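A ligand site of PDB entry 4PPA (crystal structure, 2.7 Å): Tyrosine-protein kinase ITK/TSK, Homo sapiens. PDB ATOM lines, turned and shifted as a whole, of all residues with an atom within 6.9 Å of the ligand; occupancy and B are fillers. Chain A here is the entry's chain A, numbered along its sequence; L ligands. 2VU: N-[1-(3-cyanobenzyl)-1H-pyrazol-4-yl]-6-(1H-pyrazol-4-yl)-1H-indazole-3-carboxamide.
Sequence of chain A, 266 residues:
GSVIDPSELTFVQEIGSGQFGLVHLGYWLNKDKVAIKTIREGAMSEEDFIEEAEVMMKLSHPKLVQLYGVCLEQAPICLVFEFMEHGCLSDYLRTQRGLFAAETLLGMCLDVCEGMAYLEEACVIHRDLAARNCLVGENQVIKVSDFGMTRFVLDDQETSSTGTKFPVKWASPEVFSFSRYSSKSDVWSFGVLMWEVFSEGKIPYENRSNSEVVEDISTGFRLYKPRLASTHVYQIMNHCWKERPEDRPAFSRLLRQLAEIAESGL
The side-chain amide oxygen (OD1) of Asn 133 lies close to the side-chain carboxylate (OD2) of Asp 146, 3.0 Å away.
The side-chain hydroxyl (OG) of Ser 145 is in hydrogen-bond range of the backbone carbonyl oxygen (O) of Asn 133, at 2.7 Å.
NZ of Lys 33 is in salt-bridge range of OE2 of Glu 85 (3.8 Å).
The backbone NH (N) of Glu 82 sits at hydrogen-bond distance from the backbone carbonyl oxygen (O) of Gln 66, 2.8 Å away.
The side-chain amino group (NZ) of Lys 37 is in salt-bridge range of the side-chain carboxylate (OD1) of Asp 146.
N of Val 65 lies within hydrogen-bond range of O of Val 144 (3.0 Å).
The backbone NH of Val 136 sits at hydrogen-bond distance from the backbone carbonyl oxygen of Gly 87 (2.9 Å).
The backbone carbonyl oxygen (O) of Ala 35 sits at hydrogen-bond distance from the backbone NH (N) of Phe 81 (2.8 Å).
Ala 35 touches the ligand (CB to N25, 3.3 Å).
Val 65 touches the ligand (CG1 to C29, 3.8 Å).
CZ of Phe 81 touches N30 of the ligand, 3.4 Å away.
Phe 83 touches the ligand.
O of Glu 85 touches C9 of the ligand, at 3.4 Å.
Gly 87 touches the ligand (N to C11, 3.5 Å).
CD1 of Leu 135 touches C24 of the ligand (3.5 Å).
Ser 145 touches the ligand (CB to C29, 3.6 Å).
Hydrophobic or aromatic side chains within 4 Å of the ligand: Ala 35, Val 65, Phe 81, Phe 83, Met 84 and Leu 135.
13 residues have an atom within 4 Å of the ligand: Lys 33, Ala 35, Lys 37, Val 65, Phe 81, Glu 82, Phe 83, Met 84, Glu 85, Gly 87, Leu 135, Ser 145 and Asp 146.
The nearest printed residue that does not touch the ligand is His 86 (4.3 Å).
The side-chain amino group (NZ) of Lys 37 lies within hydrogen-bond range of a nitrogen (N32) of the ligand.
The backbone carbonyl oxygen (O) of Met 84 lies within hydrogen-bond range of a nitrogen (N15) of the ligand, 2.8 Å away.
N8 of the ligand is in hydrogen-bond range of NZ of Lys 33, 3.2 Å away.
The side-chain carboxylate (OD1) of Asp 146 lies close to a nitrogen (N32) of the ligand (3.1 Å).
The backbone NH (N) of Asp 146 sits close to a nitrogen (N30) of the ligand, 3.5 Å away.
A nitrogen (N27) of the ligand sits at hydrogen-bond distance from the backbone NH (N) of Met 84 (3.0 Å).
The backbone carbonyl oxygen of Glu 82 lies within hydrogen-bond range of a nitrogen (N25) of the ligand (2.8 Å).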
ATOM      1  N   LYS A  33      -2.131  27.148 -21.392  1.00  0.00           N
ATOM      2  CA  LYS A  33      -3.062  28.013 -20.643  1.00  0.00           C
ATOM      3  C   LYS A  33      -3.125  27.527 -19.190  1.00  0.00           C
ATOM      4  O   LYS A  33      -3.235  26.321 -18.939  1.00  0.00           O
ATOM      5  CB  LYS A  33      -4.477  27.939 -21.236  1.00  0.00           C
ATOM      6  CG  LYS A  33      -4.712  28.765 -22.475  1.00  0.00           C
ATOM      7  CD  LYS A  33      -6.157  28.666 -22.920  1.00  0.00           C
ATOM      8  CE  LYS A  33      -6.371  29.224 -24.297  1.00  0.00           C
ATOM      9  NZ  LYS A  33      -7.729  28.899 -24.810  1.00  0.00           N
ATOM     10  N   VAL A  34      -3.021  28.463 -18.238  1.00  0.00           N
ATOM     11  CA  VAL A  34      -3.091  28.214 -16.801  1.00  0.00           C
ATOM     12  C   VAL A  34      -3.951  29.274 -16.125  1.00  0.00           C
ATOM     13  O   VAL A  34      -4.137  30.360 -16.663  1.00  0.00           O
ATOM     14  CB  VAL A  34      -1.691  28.113 -16.110  1.00  0.00           C
ATOM     15  CG1 VAL A  34      -0.984  26.803 -16.441  1.00  0.00           C
ATOM     16  CG2 VAL A  34      -0.804  29.323 -16.404  1.00  0.00           C
ATOM     17  N   ALA A  35      -4.460  28.959 -14.915  1.00  0.00           N
ATOM     18  CA  ALA A  35      -5.199  29.926 -14.100  1.00  0.00           C
ATOM     19  C   ALA A  35      -4.285  30.280 -12.930  1.00  0.00           C
ATOM     20  O   ALA A  35      -3.844  29.389 -12.200  1.00  0.00           O
ATOM     21  CB  ALA A  35      -6.496  29.325 -13.597  1.00  0.00           C
ATOM     22  N   ILE A  36      -3.928  31.560 -12.806  1.00  0.00           N
ATOM     23  CA  ILE A  36      -3.009  32.043 -11.769  1.00  0.00           C
ATOM     24  C   ILE A  36      -3.777  32.798 -10.671  1.00  0.00           C
ATOM     25  O   ILE A  36      -4.353  33.859 -10.928  1.00  0.00           O
ATOM     26  CB  ILE A  36      -1.803  32.857 -12.345  1.00  0.00           C
ATOM     27  CG1 ILE A  36      -1.195  32.190 -13.605  1.00  0.00           C
ATOM     28  CG2 ILE A  36      -0.744  33.075 -11.271  1.00  0.00           C
ATOM     29  CD1 ILE A  36      -0.468  33.143 -14.575  1.00  0.00           C
ATOM     30  N   LYS A  37      -3.741  32.241  -9.443  1.00  0.00           N
ATOM     31  CA  LYS A  37      -4.396  32.795  -8.261  1.00  0.00           C
ATOM     32  C   LYS A  37      -3.371  33.591  -7.437  1.00  0.00           C
ATOM     33  O   LYS A  37      -2.389  33.016  -6.959  1.00  0.00           O
ATOM     34  CB  LYS A  37      -5.004  31.641  -7.436  1.00  0.00           C
ATOM     35  CG  LYS A  37      -6.011  32.045  -6.355  1.00  0.00           C
ATOM     36  CD  LYS A  37      -6.404  30.822  -5.520  1.00  0.00           C
ATOM     37  CE  LYS A  37      -7.366  31.115  -4.396  1.00  0.00           C
ATOM     38  NZ  LYS A  37      -8.766  31.299  -4.876  1.00  0.00           N
ATOM     39  N   MET A  56      -0.931  19.747  -1.369  1.00  0.00           N
ATOM     40  CA  MET A  56      -2.030  19.963  -2.323  1.00  0.00           C
ATOM     41  C   MET A  56      -1.683  19.325  -3.687  1.00  0.00           C
ATOM     42  O   MET A  56      -2.563  18.761  -4.341  1.00  0.00           O
ATOM     43  CB  MET A  56      -2.339  21.470  -2.464  1.00  0.00           C
ATOM     44  CG  MET A  56      -3.498  21.795  -3.392  1.00  0.00           C
ATOM     45  SD  MET A  56      -4.724  22.964  -2.721  1.00  0.00           S
ATOM     46  CE  MET A  56      -3.745  24.470  -2.613  1.00  0.00           C
ATOM     47  N   VAL A  65      -9.422  20.250  -9.519  1.00  0.00           N
ATOM     48  CA  VAL A  65      -8.546  21.183 -10.242  1.00  0.00           C
ATOM     49  C   VAL A  65      -7.118  20.939  -9.727  1.00  0.00           C
ATOM     50  O   VAL A  65      -6.901  20.806  -8.510  1.00  0.00           O
ATOM     51  CB  VAL A  65      -9.007  22.657 -10.122  1.00  0.00           C
ATOM     52  CG1 VAL A  65      -8.665  23.264  -8.761  1.00  0.00           C
ATOM     53  CG2 VAL A  65      -8.409  23.504 -11.247  1.00  0.00           C
ATOM     54  N   GLN A  66      -6.163  20.785 -10.641  1.00  0.00           N
ATOM     55  CA  GLN A  66      -4.786  20.491 -10.254  1.00  0.00           C
ATOM     56  C   GLN A  66      -3.937  21.746 -10.030  1.00  0.00           C
ATOM     57  O   GLN A  66      -4.084  22.727 -10.760  1.00  0.00           O
ATOM     58  CB  GLN A  66      -4.124  19.524 -11.258  1.00  0.00           C
ATOM     59  CG  GLN A  66      -2.859  18.822 -10.749  1.00  0.00           C
ATOM     60  CD  GLN A  66      -3.114  17.755  -9.711  1.00  0.00           C
ATOM     61  OE1 GLN A  66      -2.724  17.880  -8.541  1.00  0.00           O
ATOM     62  NE2 GLN A  66      -3.759  16.668 -10.119  1.00  0.00           N
ATOM     63  N   PHE A  81      -2.511  27.079 -11.334  1.00  0.00           N
ATOM     64  CA  PHE A  81      -3.514  26.017 -11.403  1.00  0.00           C
ATOM     65  C   PHE A  81      -3.830  25.604 -12.830  1.00  0.00           C
ATOM     66  O   PHE A  81      -3.512  26.321 -13.791  1.00  0.00           O
ATOM     67  CB  PHE A  81      -4.824  26.486 -10.728  1.00  0.00           C
ATOM     68  CG  PHE A  81      -4.797  26.594  -9.232  1.00  0.00           C
ATOM     69  CD1 PHE A  81      -4.790  27.837  -8.603  1.00  0.00           C
ATOM     70  CD2 PHE A  81      -4.826  25.459  -8.430  1.00  0.00           C
ATOM     71  CE1 PHE A  81      -4.780  27.944  -7.215  1.00  0.00           C
ATOM     72  CE2 PHE A  81      -4.828  25.565  -7.035  1.00  0.00           C
ATOM     73  CZ  PHE A  81      -4.796  26.805  -6.433  1.00  0.00           C
ATOM     74  N   GLU A  82      -4.524  24.467 -12.950  1.00  0.00           N
ATOM     75  CA  GLU A  82      -5.051  23.907 -14.187  1.00  0.00           C
ATOM     76  C   GLU A  82      -6.122  24.868 -14.698  1.00  0.00           C
ATOM     77  O   GLU A  82      -6.930  25.374 -13.911  1.00  0.00           O
ATOM     78  CB  GLU A  82      -5.671  22.541 -13.865  1.00  0.00           C
ATOM     79  CG  GLU A  82      -6.404  21.868 -15.019  1.00  0.00           C
ATOM     80  CD  GLU A  82      -7.227  20.661 -14.622  1.00  0.00           C
ATOM     81  OE1 GLU A  82      -8.005  20.179 -15.475  1.00  0.00           O
ATOM     82  OE2 GLU A  82      -7.089  20.179 -13.475  1.00  0.00           O
ATOM     83  N   PHE A  83      -6.111  25.144 -16.010  1.00  0.00           N
ATOM     84  CA  PHE A  83      -7.115  26.034 -16.571  1.00  0.00           C
ATOM     85  C   PHE A  83      -8.399  25.286 -16.867  1.00  0.00           C
ATOM     86  O   PHE A  83      -8.369  24.203 -17.456  1.00  0.00           O
ATOM     87  CB  PHE A  83      -6.604  26.787 -17.807  1.00  0.00           C
ATOM     88  CG  PHE A  83      -7.549  27.855 -18.302  1.00  0.00           C
ATOM     89  CD1 PHE A  83      -7.789  29.003 -17.560  1.00  0.00           C
ATOM     90  CD2 PHE A  83      -8.186  27.727 -19.530  1.00  0.00           C
ATOM     91  CE1 PHE A  83      -8.661  29.990 -18.017  1.00  0.00           C
ATOM     92  CE2 PHE A  83      -9.051  28.715 -20.003  1.00  0.00           C
ATOM     93  CZ  PHE A  83      -9.286  29.839 -19.243  1.00  0.00           C
ATOM     94  N   MET A  84      -9.532  25.862 -16.414  1.00  0.00           N
ATOM     95  CA  MET A  84     -10.857  25.302 -16.616  1.00  0.00           C
ATOM     96  C   MET A  84     -11.603  26.203 -17.591  1.00  0.00           C
ATOM     97  O   MET A  84     -12.055  27.285 -17.234  1.00  0.00           O
ATOM     98  CB  MET A  84     -11.593  25.118 -15.283  1.00  0.00           C
ATOM     99  CG  MET A  84     -10.941  24.101 -14.355  1.00  0.00           C
ATOM    100  SD  MET A  84     -10.745  22.432 -15.030  1.00  0.00           S
ATOM    101  CE  MET A  84     -12.413  21.864 -14.978  1.00  0.00           C
ATOM    102  N   GLU A  85     -11.679  25.759 -18.854  1.00  0.00           N
ATOM    103  CA  GLU A  85     -12.251  26.403 -20.040  1.00  0.00           C
ATOM    104  C   GLU A  85     -13.552  27.215 -19.860  1.00  0.00           C
ATOM    105  O   GLU A  85     -13.657  28.264 -20.501  1.00  0.00           O
ATOM    106  CB  GLU A  85     -12.468  25.340 -21.136  1.00  0.00           C
ATOM    107  CG  GLU A  85     -12.436  25.872 -22.566  1.00  0.00           C
ATOM    108  CD  GLU A  85     -11.083  26.293 -23.112  1.00  0.00           C
ATOM    109  OE1 GLU A  85     -10.067  25.620 -22.821  1.00  0.00           O
ATOM    110  OE2 GLU A  85     -11.038  27.288 -23.868  1.00  0.00           O
ATOM    111  N   HIS A  86     -14.524  26.747 -19.049  1.00  0.00           N
ATOM    112  CA  HIS A  86     -15.831  27.412 -18.952  1.00  0.00           C
ATOM    113  C   HIS A  86     -16.172  28.125 -17.621  1.00  0.00           C
ATOM    114  O   HIS A  86     -17.342  28.443 -17.398  1.00  0.00           O
ATOM    115  CB  HIS A  86     -16.958  26.434 -19.326  1.00  0.00           C
ATOM    116  CG  HIS A  86     -16.780  25.782 -20.654  1.00  0.00           C
ATOM    117  ND1 HIS A  86     -16.729  26.519 -21.823  1.00  0.00           N
ATOM    118  CD2 HIS A  86     -16.607  24.474 -20.953  1.00  0.00           C
ATOM    119  CE1 HIS A  86     -16.543  25.640 -22.800  1.00  0.00           C
ATOM    120  NE2 HIS A  86     -16.467  24.389 -22.327  1.00  0.00           N
ATOM    121  N   GLY A  87     -15.170  28.413 -16.788  1.00  0.00           N
ATOM    122  CA  GLY A  87     -15.374  29.115 -15.521  1.00  0.00           C
ATOM    123  C   GLY A  87     -16.149  28.371 -14.450  1.00  0.00           C
ATOM    124  O   GLY A  87     -16.289  27.144 -14.516  1.00  0.00           O
ATOM    125  N   CYS A  88     -16.659  29.127 -13.446  1.00  0.00           N
ATOM    126  CA  CYS A  88     -17.403  28.554 -12.316  1.00  0.00           C
ATOM    127  C   CYS A  88     -18.753  27.974 -12.719  1.00  0.00           C
ATOM    128  O   CYS A  88     -19.406  28.498 -13.628  1.00  0.00           O
ATOM    129  CB  CYS A  88     -17.513  29.548 -11.162  1.00  0.00           C
ATOM    130  SG  CYS A  88     -18.633  30.941 -11.475  1.00  0.00           S
ATOM    131  N   ASN A 133     -17.408  27.281  -6.359  1.00  0.00           N
ATOM    132  CA  ASN A 133     -16.079  26.732  -6.112  1.00  0.00           C
ATOM    133  C   ASN A 133     -15.820  25.493  -6.984  1.00  0.00           C
ATOM    134  O   ASN A 133     -14.779  24.846  -6.849  1.00  0.00           O
ATOM    135  CB  ASN A 133     -15.891  26.424  -4.621  1.00  0.00           C
ATOM    136  CG  ASN A 133     -15.651  27.660  -3.783  1.00  0.00           C
ATOM    137  OD1 ASN A 133     -14.688  28.406  -3.997  1.00  0.00           O
ATOM    138  ND2 ASN A 133     -16.512  27.886  -2.802  1.00  0.00           N
ATOM    139  N   LEU A 135     -15.653  24.073 -11.034  1.00  0.00           N
ATOM    140  CA  LEU A 135     -15.355  24.631 -12.344  1.00  0.00           C
ATOM    141  C   LEU A 135     -15.657  23.694 -13.491  1.00  0.00           C
ATOM    142  O   LEU A 135     -15.502  22.482 -13.340  1.00  0.00           O
ATOM    143  CB  LEU A 135     -13.905  25.120 -12.421  1.00  0.00           C
ATOM    144  CG  LEU A 135     -13.486  26.193 -11.441  1.00  0.00           C
ATOM    145  CD1 LEU A 135     -12.082  25.999 -11.049  1.00  0.00           C
ATOM    146  CD2 LEU A 135     -13.709  27.574 -12.008  1.00  0.00           C
ATOM    147  N   VAL A 136     -16.056  24.271 -14.640  1.00  0.00           N
ATOM    148  CA  VAL A 136     -16.409  23.550 -15.875  1.00  0.00           C
ATOM    149  C   VAL A 136     -15.237  23.552 -16.875  1.00  0.00           C
ATOM    150  O   VAL A 136     -14.672  24.614 -17.170  1.00  0.00           O
ATOM    151  CB  VAL A 136     -17.729  24.087 -16.510  1.00  0.00           C
ATOM    152  CG1 VAL A 136     -18.316  23.085 -17.506  1.00  0.00           C
ATOM    153  CG2 VAL A 136     -18.764  24.443 -15.441  1.00  0.00           C
ATOM    154  N   VAL A 144     -13.517  20.139  -8.664  1.00  0.00           N
ATOM    155  CA  VAL A 144     -13.611  20.894  -7.414  1.00  0.00           C
ATOM    156  C   VAL A 144     -12.371  21.765  -7.195  1.00  0.00           C
ATOM    157  O   VAL A 144     -11.255  21.307  -7.446  1.00  0.00           O
ATOM    158  CB  VAL A 144     -13.906  19.983  -6.190  1.00  0.00           C
ATOM    159  CG1 VAL A 144     -14.357  20.796  -4.992  1.00  0.00           C
ATOM    160  CG2 VAL A 144     -14.948  18.901  -6.523  1.00  0.00           C
ATOM    161  N   SER A 145     -12.564  23.015  -6.711  1.00  0.00           N
ATOM    162  CA  SER A 145     -11.497  23.972  -6.408  1.00  0.00           C
ATOM    163  C   SER A 145     -11.654  24.567  -5.016  1.00  0.00           C
ATOM    164  O   SER A 145     -12.696  24.347  -4.385  1.00  0.00           O
ATOM    165  CB  SER A 145     -11.437  25.060  -7.474  1.00  0.00           C
ATOM    166  OG  SER A 145     -12.433  26.051  -7.314  1.00  0.00           O
ATOM    167  N   ASP A 146     -10.629  25.310  -4.531  1.00  0.00           N
ATOM    168  CA  ASP A 146     -10.563  25.990  -3.225  1.00  0.00           C
ATOM    169  C   ASP A 146     -10.717  25.035  -2.037  1.00  0.00           C
ATOM    170  O   ASP A 146     -11.417  25.358  -1.066  1.00  0.00           O
ATOM    171  CB  ASP A 146     -11.568  27.168  -3.146  1.00  0.00           C
ATOM    172  CG  ASP A 146     -11.099  28.467  -3.771  1.00  0.00           C
ATOM    173  OD1 ASP A 146     -10.064  29.007  -3.315  1.00  0.00           O
ATOM    174  OD2 ASP A 146     -11.805  28.982  -4.671  1.00  0.00           O
ATOM    175  N   PHE A 147     -10.055  23.870  -2.085  1.00  0.00           N
ATOM    176  CA  PHE A 147     -10.134  22.879  -1.009  1.00  0.00           C
ATOM    177  C   PHE A 147      -8.971  22.987  -0.013  1.00  0.00           C
ATOM    178  O   PHE A 147      -7.851  23.330  -0.407  1.00  0.00           O
ATOM    179  CB  PHE A 147     -10.301  21.435  -1.522  1.00  0.00           C
ATOM    180  CG  PHE A 147      -9.451  21.011  -2.696  1.00  0.00           C
ATOM    181  CD1 PHE A 147      -8.229  20.380  -2.497  1.00  0.00           C
ATOM    182  CD2 PHE A 147      -9.896  21.193  -4.001  1.00  0.00           C
ATOM    183  CE1 PHE A 147      -7.459  19.959  -3.583  1.00  0.00           C
ATOM    184  CE2 PHE A 147      -9.125  20.771  -5.087  1.00  0.00           C
ATOM    185  CZ  PHE A 147      -7.904  20.161  -4.874  1.00  0.00           C
HETATM  186  C1  2VU L   1     -11.523  34.508 -20.671  1.00  0.00           C
HETATM  187  C2  2VU L   1     -12.517  33.742 -20.057  1.00  0.00           C
HETATM  188  C3  2VU L   1     -12.572  32.365 -20.277  1.00  0.00           C
HETATM  189  C4  2VU L   1     -11.623  31.750 -21.094  1.00  0.00           C
HETATM  190  C5  2VU L   1     -10.623  32.515 -21.699  1.00  0.00           C
HETATM  191  C6  2VU L   1     -10.573  33.907 -21.486  1.00  0.00           C
HETATM  192  C7  2VU L   1      -9.649  31.883 -22.545  1.00  0.00           C
HETATM  193  N8  2VU L   1      -8.887  31.377 -23.218  1.00  0.00           N
HETATM  194  C9  2VU L   1     -13.643  31.529 -19.623  1.00  0.00           C
HETATM  195  N10 2VU L   1     -13.224  31.274 -18.249  1.00  0.00           N
HETATM  196  C11 2VU L   1     -12.413  30.263 -17.840  1.00  0.00           C
HETATM  197  C12 2VU L   1     -12.228  30.400 -16.501  1.00  0.00           C
HETATM  198  C13 2VU L   1     -12.908  31.568 -16.108  1.00  0.00           C
HETATM  199  N14 2VU L   1     -13.502  32.087 -17.150  1.00  0.00           N
HETATM  200  N15 2VU L   1     -11.433  29.542 -15.696  1.00  0.00           N
HETATM  201  C16 2VU L   1     -11.166  29.740 -14.379  1.00  0.00           C
HETATM  202  O17 2VU L   1     -11.652  30.679 -13.777  1.00  0.00           O
HETATM  203  C18 2VU L   1     -10.292  28.806 -13.644  1.00  0.00           C
HETATM  204  C19 2VU L   1     -10.053  28.824 -12.198  1.00  0.00           C
HETATM  205  C20 2VU L   1     -10.490  29.625 -11.140  1.00  0.00           C
HETATM  206  C21 2VU L   1     -10.066  29.367  -9.866  1.00  0.00           C
HETATM  207  C22 2VU L   1      -9.178  28.290  -9.609  1.00  0.00           C
HETATM  208  C23 2VU L   1      -8.741  27.467 -10.656  1.00  0.00           C
HETATM  209  C24 2VU L   1      -9.174  27.729 -11.972  1.00  0.00           C
HETATM  210  N25 2VU L   1      -8.961  27.166 -13.206  1.00  0.00           N
HETATM  211  N27 2VU L   1      -9.603  27.792 -14.134  1.00  0.00           N
HETATM  212  C28 2VU L   1      -8.808  28.014  -8.183  1.00  0.00           C
HETATM  213  C29 2VU L   1      -8.301  26.852  -7.678  1.00  0.00           C
HETATM  214  N30 2VU L   1      -8.173  26.995  -6.338  1.00  0.00           N
HETATM  215  N32 2VU L   1      -8.626  28.271  -5.994  1.00  0.00           N
HETATM  216  C33 2VU L   1      -9.022  28.870  -7.083  1.00  0.00           C
